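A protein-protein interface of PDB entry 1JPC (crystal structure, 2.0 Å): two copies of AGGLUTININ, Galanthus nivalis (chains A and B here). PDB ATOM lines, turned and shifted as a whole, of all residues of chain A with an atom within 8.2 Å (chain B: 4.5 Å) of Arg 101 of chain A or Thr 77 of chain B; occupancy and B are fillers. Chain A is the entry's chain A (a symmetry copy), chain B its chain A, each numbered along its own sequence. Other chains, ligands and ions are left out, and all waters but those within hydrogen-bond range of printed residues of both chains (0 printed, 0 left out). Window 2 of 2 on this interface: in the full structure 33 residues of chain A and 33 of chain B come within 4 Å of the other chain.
NE of Arg 101 of chain A is in hydrogen-bond range of O of Gly 98 of chain B, at 2.9 Å. NE of Arg 101 of chain B lies within hydrogen-bond range of O of Gly 98 of chain A (2.9 Å). N of Ile 96 of chain B sits at hydrogen-bond distance from O of Trp 102 of chain A, 3.0 Å away. NH2 of Arg 101 of chain A sits close to NH2 of Arg 101 of chain B, 3.3 Å away. The backbone carbonyl oxygen of Ile 96 of chain B lies within hydrogen-bond range of the backbone NH of Arg 101 of chain A. O of Gly 98 of chain A lies close to O of Gly 98 of chain B. The backbone NH (N) of Gly 98 of chain B sits at hydrogen-bond distance from the backbone carbonyl oxygen (O) of Thr 99 of chain A (3.3 Å).
The side-chain hydroxyl (OG1) of Thr 77 of chain B lies within hydrogen-bond range of the backbone carbonyl oxygen (O) of Gly 60 of chain B (2.8 Å). The side-chain hydroxyl (OG) of Ser 75 of chain B lies within hydrogen-bond range of the side-chain hydroxyl (OG1) of Thr 77 of chain B, at 2.7 Å. O of Leu 62 of chain B lies within hydrogen-bond range of N of Ser 75 of chain B (3.0 Å). OD1 of Asp 100 of chain A is in hydrogen-bond range of ND2 of Asn 83 of chain A. The side-chain hydroxyl (OG) of Ser 75 of chain B is in hydrogen-bond range of the side-chain amide oxygen (OD1) of Asn 61 of chain B, at 3.2 Å. NE of Arg 101 of chain A is in hydrogen-bond range of O of Thr 99 of chain A, 3.4 Å away.
Ile 96 of chain B touches Asp 100 of chain A. Arg 101 of chain A touches Thr 77 of chain B. Trp 102 of chain A touches Ser 75 of chain B. Trp 102 of chain A touches Thr 77 of chain B (CB to CG2, 3.4 Å).
Arg 101 of chain A touches four residues of chain B. Thr 77 of chain B touches just these residues of chain A: Arg 101 (3.4 Å) and Trp 102 (3.4 Å). No residue of chain A comes within 4 Å of Gly 78 of chain B. Of the printed residues of chain B, Gly 98 of chain A touches Gly 98 and Arg 101. Of the printed residues of chain B, Thr 99 of chain A touches Gly 98 (3.3 Å). Of the printed residues of chain A, Gly 98 of chain B touches Gly 98, Thr 99 and Arg 101. Printed residues of chain A within 4 Å of Ser 75 of chain B: Trp 102 (3.7 Å).
Of the 12 printed residues of chain B, 5 touch a printed residue of chain A. Hydrophobic or aromatic side chains of chain B within 4 Å of the printed part of chain A: Ile 96. Along chain B the printed residues that touch a printed residue of chain A span positions 75 to 101. Hydrophobic or aromatic side chains of chain A within 4 Å of the printed part of chain B: Trp 102. Along chain A the printed residues that touch a printed residue of chain B span positions 98 to 102. Among the printed residues, 11 pairs touch across the chains. Among the printed residues, no Asp or Glu carboxylate lies within 4 Å of a Lys or Arg side-chain nitrogen of the other chain.
Gly 98 of chain A touches its own counterpart, Gly 98 of chain B. Gly 98 of chain A touches Arg 101 of chain B, and with the chains exchanged Arg 101 of chain A touches Gly 98 of chain B. Arg 101 of chain B touches its own counterpart, Arg 101 of chain A. Positions printed for both chains: 98 and 101. Of the 11 pairs that touch across the chains among the printed residues, 4 have their exchanged pair printed and touching as well.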
ATOM      1  N   GLN A  80     -31.424  10.345 -10.157  1.00  0.00           N
ATOM      2  CA  GLN A  80     -32.560  10.745 -10.973  1.00  0.00           C
ATOM      3  C   GLN A  80     -33.323   9.539 -11.520  1.00  0.00           C
ATOM      4  O   GLN A  80     -32.726   8.555 -11.941  1.00  0.00           O
ATOM      5  CB  GLN A  80     -32.060  11.623 -12.116  1.00  0.00           C
ATOM      6  CG  GLN A  80     -33.143  12.345 -12.879  1.00  0.00           C
ATOM      7  CD  GLN A  80     -32.594  13.543 -13.621  1.00  0.00           C
ATOM      8  OE1 GLN A  80     -31.398  13.833 -13.553  1.00  0.00           O
ATOM      9  NE2 GLN A  80     -33.464  14.259 -14.317  1.00  0.00           N
ATOM     10  N   ASN A  83     -34.413   6.327 -17.535  1.00  0.00           N
ATOM     11  CA  ASN A  83     -34.004   5.124 -18.257  1.00  0.00           C
ATOM     12  C   ASN A  83     -32.491   5.053 -18.288  1.00  0.00           C
ATOM     13  O   ASN A  83     -31.835   6.031 -18.628  1.00  0.00           O
ATOM     14  CB  ASN A  83     -34.545   5.152 -19.685  1.00  0.00           C
ATOM     15  CG  ASN A  83     -36.054   5.226 -19.726  1.00  0.00           C
ATOM     16  OD1 ASN A  83     -36.737   4.297 -19.313  1.00  0.00           O
ATOM     17  ND2 ASN A  83     -36.581   6.343 -20.204  1.00  0.00           N
ATOM     18  N   TYR A  84     -31.957   3.897 -17.903  1.00  0.00           N
ATOM     19  CA  TYR A  84     -30.516   3.653 -17.858  1.00  0.00           C
ATOM     20  C   TYR A  84     -30.194   2.304 -18.481  1.00  0.00           C
ATOM     21  O   TYR A  84     -31.082   1.450 -18.630  1.00  0.00           O
ATOM     22  CB  TYR A  84     -30.025   3.609 -16.407  1.00  0.00           C
ATOM     23  CG  TYR A  84     -30.209   4.894 -15.650  1.00  0.00           C
ATOM     24  CD1 TYR A  84     -31.402   5.173 -14.979  1.00  0.00           C
ATOM     25  CD2 TYR A  84     -29.185   5.833 -15.593  1.00  0.00           C
ATOM     26  CE1 TYR A  84     -31.565   6.360 -14.274  1.00  0.00           C
ATOM     27  CE2 TYR A  84     -29.334   7.017 -14.894  1.00  0.00           C
ATOM     28  CZ  TYR A  84     -30.522   7.274 -14.239  1.00  0.00           C
ATOM     29  OH  TYR A  84     -30.658   8.459 -13.569  1.00  0.00           O
ATOM     30  N   TYR A  97     -24.835   4.028 -18.375  1.00  0.00           N
ATOM     31  CA  TYR A  97     -25.084   5.311 -19.028  1.00  0.00           C
ATOM     32  C   TYR A  97     -26.538   5.670 -18.778  1.00  0.00           C
ATOM     33  O   TYR A  97     -27.394   4.782 -18.670  1.00  0.00           O
ATOM     34  CB  TYR A  97     -24.885   5.250 -20.549  1.00  0.00           C
ATOM     35  CG  TYR A  97     -23.475   5.032 -21.041  1.00  0.00           C
ATOM     36  CD1 TYR A  97     -22.980   3.744 -21.239  1.00  0.00           C
ATOM     37  CD2 TYR A  97     -22.663   6.109 -21.379  1.00  0.00           C
ATOM     38  CE1 TYR A  97     -21.713   3.537 -21.765  1.00  0.00           C
ATOM     39  CE2 TYR A  97     -21.390   5.916 -21.904  1.00  0.00           C
ATOM     40  CZ  TYR A  97     -20.923   4.629 -22.096  1.00  0.00           C
ATOM     41  OH  TYR A  97     -19.667   4.436 -22.616  1.00  0.00           O
ATOM     42  N   GLY A  98     -26.822   6.966 -18.718  1.00  0.00           N
ATOM     43  CA  GLY A  98     -28.186   7.418 -18.502  1.00  0.00           C
ATOM     44  C   GLY A  98     -28.223   8.872 -18.079  1.00  0.00           C
ATOM     45  O   GLY A  98     -27.202   9.413 -17.645  1.00  0.00           O
ATOM     46  N   THR A  99     -29.373   9.521 -18.210  1.00  0.00           N
ATOM     47  CA  THR A  99     -30.583   8.912 -18.740  1.00  0.00           C
ATOM     48  C   THR A  99     -30.633   9.087 -20.252  1.00  0.00           C
ATOM     49  O   THR A  99     -29.662   9.527 -20.866  1.00  0.00           O
ATOM     50  CB  THR A  99     -31.834   9.592 -18.139  1.00  0.00           C
ATOM     51  OG1 THR A  99     -31.668  11.015 -18.192  1.00  0.00           O
ATOM     52  CG2 THR A  99     -32.049   9.169 -16.698  1.00  0.00           C
ATOM     53  N   ASP A 100     -31.766   8.725 -20.845  1.00  0.00           N
ATOM     54  CA  ASP A 100     -31.973   8.865 -22.277  1.00  0.00           C
ATOM     55  C   ASP A 100     -32.056  10.350 -22.616  1.00  0.00           C
ATOM     56  O   ASP A 100     -32.605  11.143 -21.848  1.00  0.00           O
ATOM     57  CB  ASP A 100     -33.258   8.146 -22.696  1.00  0.00           C
ATOM     58  CG  ASP A 100     -34.454   8.541 -21.849  1.00  0.00           C
ATOM     59  OD1 ASP A 100     -34.416   8.334 -20.618  1.00  0.00           O
ATOM     60  OD2 ASP A 100     -35.443   9.050 -22.405  1.00  0.00           O
ATOM     61  N   ARG A 101     -31.474  10.734 -23.743  1.00  0.00           N
ATOM     62  CA  ARG A 101     -31.472  12.129 -24.172  1.00  0.00           C
ATOM     63  C   ARG A 101     -32.268  12.328 -25.455  1.00  0.00           C
ATOM     64  O   ARG A 101     -32.736  13.426 -25.746  1.00  0.00           O
ATOM     65  CB  ARG A 101     -30.033  12.594 -24.411  1.00  0.00           C
ATOM     66  CG  ARG A 101     -29.110  12.409 -23.221  1.00  0.00           C
ATOM     67  CD  ARG A 101     -29.615  13.193 -22.020  1.00  0.00           C
ATOM     68  NE  ARG A 101     -28.881  12.874 -20.796  1.00  0.00           N
ATOM     69  CZ  ARG A 101     -29.192  13.347 -19.590  1.00  0.00           C
ATOM     70  NH1 ARG A 101     -30.224  14.169 -19.443  1.00  0.00           N
ATOM     71  NH2 ARG A 101     -28.485  12.984 -18.526  1.00  0.00           N
ATOM     72  N   TRP A 102     -32.431  11.255 -26.216  1.00  0.00           N
ATOM     73  CA  TRP A 102     -33.123  11.307 -27.491  1.00  0.00           C
ATOM     74  C   TRP A 102     -33.509   9.877 -27.888  1.00  0.00           C
ATOM     75  O   TRP A 102     -32.848   8.916 -27.487  1.00  0.00           O
ATOM     76  CB  TRP A 102     -32.169  11.909 -28.540  1.00  0.00           C
ATOM     77  CG  TRP A 102     -32.731  12.000 -29.921  1.00  0.00           C
ATOM     78  CD1 TRP A 102     -33.481  13.019 -30.429  1.00  0.00           C
ATOM     79  CD2 TRP A 102     -32.638  11.014 -30.961  1.00  0.00           C
ATOM     80  NE1 TRP A 102     -33.873  12.725 -31.713  1.00  0.00           N
ATOM     81  CE2 TRP A 102     -33.372  11.504 -32.068  1.00  0.00           C
ATOM     82  CE3 TRP A 102     -32.012   9.760 -31.064  1.00  0.00           C
ATOM     83  CZ2 TRP A 102     -33.500  10.787 -33.266  1.00  0.00           C
ATOM     84  CZ3 TRP A 102     -32.142   9.042 -32.260  1.00  0.00           C
ATOM     85  CH2 TRP A 102     -32.882   9.564 -33.344  1.00  0.00           C
ATOM     86  N   ALA A 103     -34.579   9.747 -28.666  1.00  0.00           N
ATOM     87  CA  ALA A 103     -35.039   8.451 -29.146  1.00  0.00           C
ATOM     88  C   ALA A 103     -35.870   8.659 -30.411  1.00  0.00           C
ATOM     89  O   ALA A 103     -36.395   9.751 -30.634  1.00  0.00           O
ATOM     90  CB  ALA A 103     -35.859   7.741 -28.073  1.00  0.00           C
ATOM     91  N   ASP B  59     -20.292  15.467 -27.450  1.00  0.00           N
ATOM     92  CA  ASP B  59     -21.163  16.443 -26.793  1.00  0.00           C
ATOM     93  C   ASP B  59     -22.601  15.897 -26.741  1.00  0.00           C
ATOM     94  O   ASP B  59     -23.551  16.627 -26.439  1.00  0.00           O
ATOM     95  CB  ASP B  59     -21.109  17.820 -27.489  1.00  0.00           C
ATOM     96  CG  ASP B  59     -21.698  17.814 -28.893  1.00  0.00           C
ATOM     97  OD1 ASP B  59     -21.767  16.740 -29.525  1.00  0.00           O
ATOM     98  OD2 ASP B  59     -22.083  18.902 -29.377  1.00  0.00           O
ATOM     99  N   GLY B  60     -22.748  14.605 -27.047  1.00  0.00           N
ATOM    100  CA  GLY B  60     -24.047  13.959 -27.028  1.00  0.00           C
ATOM    101  C   GLY B  60     -24.919  14.214 -28.236  1.00  0.00           C
ATOM    102  O   GLY B  60     -26.104  13.878 -28.222  1.00  0.00           O
ATOM    103  N   ASN B  61     -24.348  14.780 -29.292  1.00  0.00           N
ATOM    104  CA  ASN B  61     -25.120  15.074 -30.493  1.00  0.00           C
ATOM    105  C   ASN B  61     -24.894  14.051 -31.609  1.00  0.00           C
ATOM    106  O   ASN B  61     -23.756  13.693 -31.926  1.00  0.00           O
ATOM    107  CB  ASN B  61     -24.790  16.485 -30.995  1.00  0.00           C
ATOM    108  CG  ASN B  61     -25.942  17.126 -31.754  1.00  0.00           C
ATOM    109  OD1 ASN B  61     -27.077  16.646 -31.710  1.00  0.00           O
ATOM    110  ND2 ASN B  61     -25.660  18.227 -32.441  1.00  0.00           N
ATOM    111  N   LEU B  62     -25.993  13.533 -32.145  1.00  0.00           N
ATOM    112  CA  LEU B  62     -25.959  12.564 -33.235  1.00  0.00           C
ATOM    113  C   LEU B  62     -26.152  13.402 -34.496  1.00  0.00           C
ATOM    114  O   LEU B  62     -27.213  14.000 -34.677  1.00  0.00           O
ATOM    115  CB  LEU B  62     -27.109  11.567 -33.071  1.00  0.00           C
ATOM    116  CG  LEU B  62     -27.131  10.386 -34.033  1.00  0.00           C
ATOM    117  CD1 LEU B  62     -25.953   9.488 -33.728  1.00  0.00           C
ATOM    118  CD2 LEU B  62     -28.427   9.622 -33.878  1.00  0.00           C
ATOM    119  N   SER B  75     -29.738  15.415 -33.947  1.00  0.00           N
ATOM    120  CA  SER B  75     -30.712  15.111 -32.913  1.00  0.00           C
ATOM    121  C   SER B  75     -30.943  16.349 -32.050  1.00  0.00           C
ATOM    122  O   SER B  75     -31.981  16.465 -31.401  1.00  0.00           O
ATOM    123  CB  SER B  75     -30.253  13.929 -32.049  1.00  0.00           C
ATOM    124  OG  SER B  75     -28.913  14.078 -31.615  1.00  0.00           O
ATOM    125  N   ASN B  76     -29.990  17.286 -32.091  1.00  0.00           N
ATOM    126  CA  ASN B  76     -30.054  18.538 -31.318  1.00  0.00           C
ATOM    127  C   ASN B  76     -30.054  18.227 -29.826  1.00  0.00           C
ATOM    128  O   ASN B  76     -30.794  18.825 -29.038  1.00  0.00           O
ATOM    129  CB  ASN B  76     -31.286  19.377 -31.691  1.00  0.00           C
ATOM    130  CG  ASN B  76     -31.315  19.764 -33.162  1.00  0.00           C
ATOM    131  OD1 ASN B  76     -30.321  20.238 -33.716  1.00  0.00           O
ATOM    132  ND2 ASN B  76     -32.461  19.564 -33.803  1.00  0.00           N
ATOM    133  N   THR B  77     -29.215  17.272 -29.446  1.00  0.00           N
ATOM    134  CA  THR B  77     -29.088  16.847 -28.066  1.00  0.00           C
ATOM    135  C   THR B  77     -27.674  17.156 -27.585  1.00  0.00           C
ATOM    136  O   THR B  77     -27.217  16.632 -26.566  1.00  0.00           O
ATOM    137  CB  THR B  77     -29.376  15.334 -27.933  1.00  0.00           C
ATOM    138  OG1 THR B  77     -28.699  14.620 -28.979  1.00  0.00           O
ATOM    139  CG2 THR B  77     -30.874  15.064 -28.019  1.00  0.00           C
ATOM    140  N   GLY B  78     -26.977  17.993 -28.352  1.00  0.00           N
ATOM    141  CA  GLY B  78     -25.629  18.382 -27.995  1.00  0.00           C
ATOM    142  C   GLY B  78     -25.670  19.110 -26.667  1.00  0.00           C
ATOM    143  O   GLY B  78     -26.660  19.782 -26.345  1.00  0.00           O
ATOM    144  N   GLY B  79     -24.615  18.966 -25.881  1.00  0.00           N
ATOM    145  CA  GLY B  79     -24.580  19.623 -24.594  1.00  0.00           C
ATOM    146  C   GLY B  79     -23.301  19.353 -23.841  1.00  0.00           C
ATOM    147  O   GLY B  79     -22.209  19.758 -24.262  1.00  0.00           O
ATOM    148  N   ILE B  96     -30.309   7.414 -27.410  1.00  0.00           N
ATOM    149  CA  ILE B  96     -28.996   7.954 -27.035  1.00  0.00           C
ATOM    150  C   ILE B  96     -29.012   8.076 -25.498  1.00  0.00           C
ATOM    151  O   ILE B  96     -29.943   8.653 -24.934  1.00  0.00           O
ATOM    152  CB  ILE B  96     -28.742   9.375 -27.621  1.00  0.00           C
ATOM    153  CG1 ILE B  96     -28.566   9.323 -29.134  1.00  0.00           C
ATOM    154  CG2 ILE B  96     -27.504  10.002 -26.991  1.00  0.00           C
ATOM    155  CD1 ILE B  96     -28.406  10.695 -29.772  1.00  0.00           C
ATOM    156  N   GLY B  98     -26.550   8.882 -21.914  1.00  0.00           N
ATOM    157  CA  GLY B  98     -25.308   9.509 -21.494  1.00  0.00           C
ATOM    158  C   GLY B  98     -25.557  10.565 -20.437  1.00  0.00           C
ATOM    159  O   GLY B  98     -26.691  11.025 -20.281  1.00  0.00           O
ATOM    160  N   ARG B 101     -22.121   7.075 -15.733  1.00  0.00           N
ATOM    161  CA  ARG B 101     -22.314   7.357 -14.315  1.00  0.00           C
ATOM    162  C   ARG B 101     -21.440   6.473 -13.436  1.00  0.00           C
ATOM    163  O   ARG B 101     -21.135   6.814 -12.296  1.00  0.00           O
ATOM    164  CB  ARG B 101     -23.779   7.129 -13.937  1.00  0.00           C
ATOM    165  CG  ARG B 101     -24.771   7.919 -14.769  1.00  0.00           C
ATOM    166  CD  ARG B 101     -24.525   9.413 -14.627  1.00  0.00           C
ATOM    167  NE  ARG B 101     -25.312  10.201 -15.575  1.00  0.00           N
ATOM    168  CZ  ARG B 101     -25.205  11.520 -15.724  1.00  0.00           C
ATOM    169  NH1 ARG B 101     -24.345  12.206 -14.982  1.00  0.00           N
ATOM    170  NH2 ARG B 101     -25.943  12.154 -16.628  1.00  0.00           N
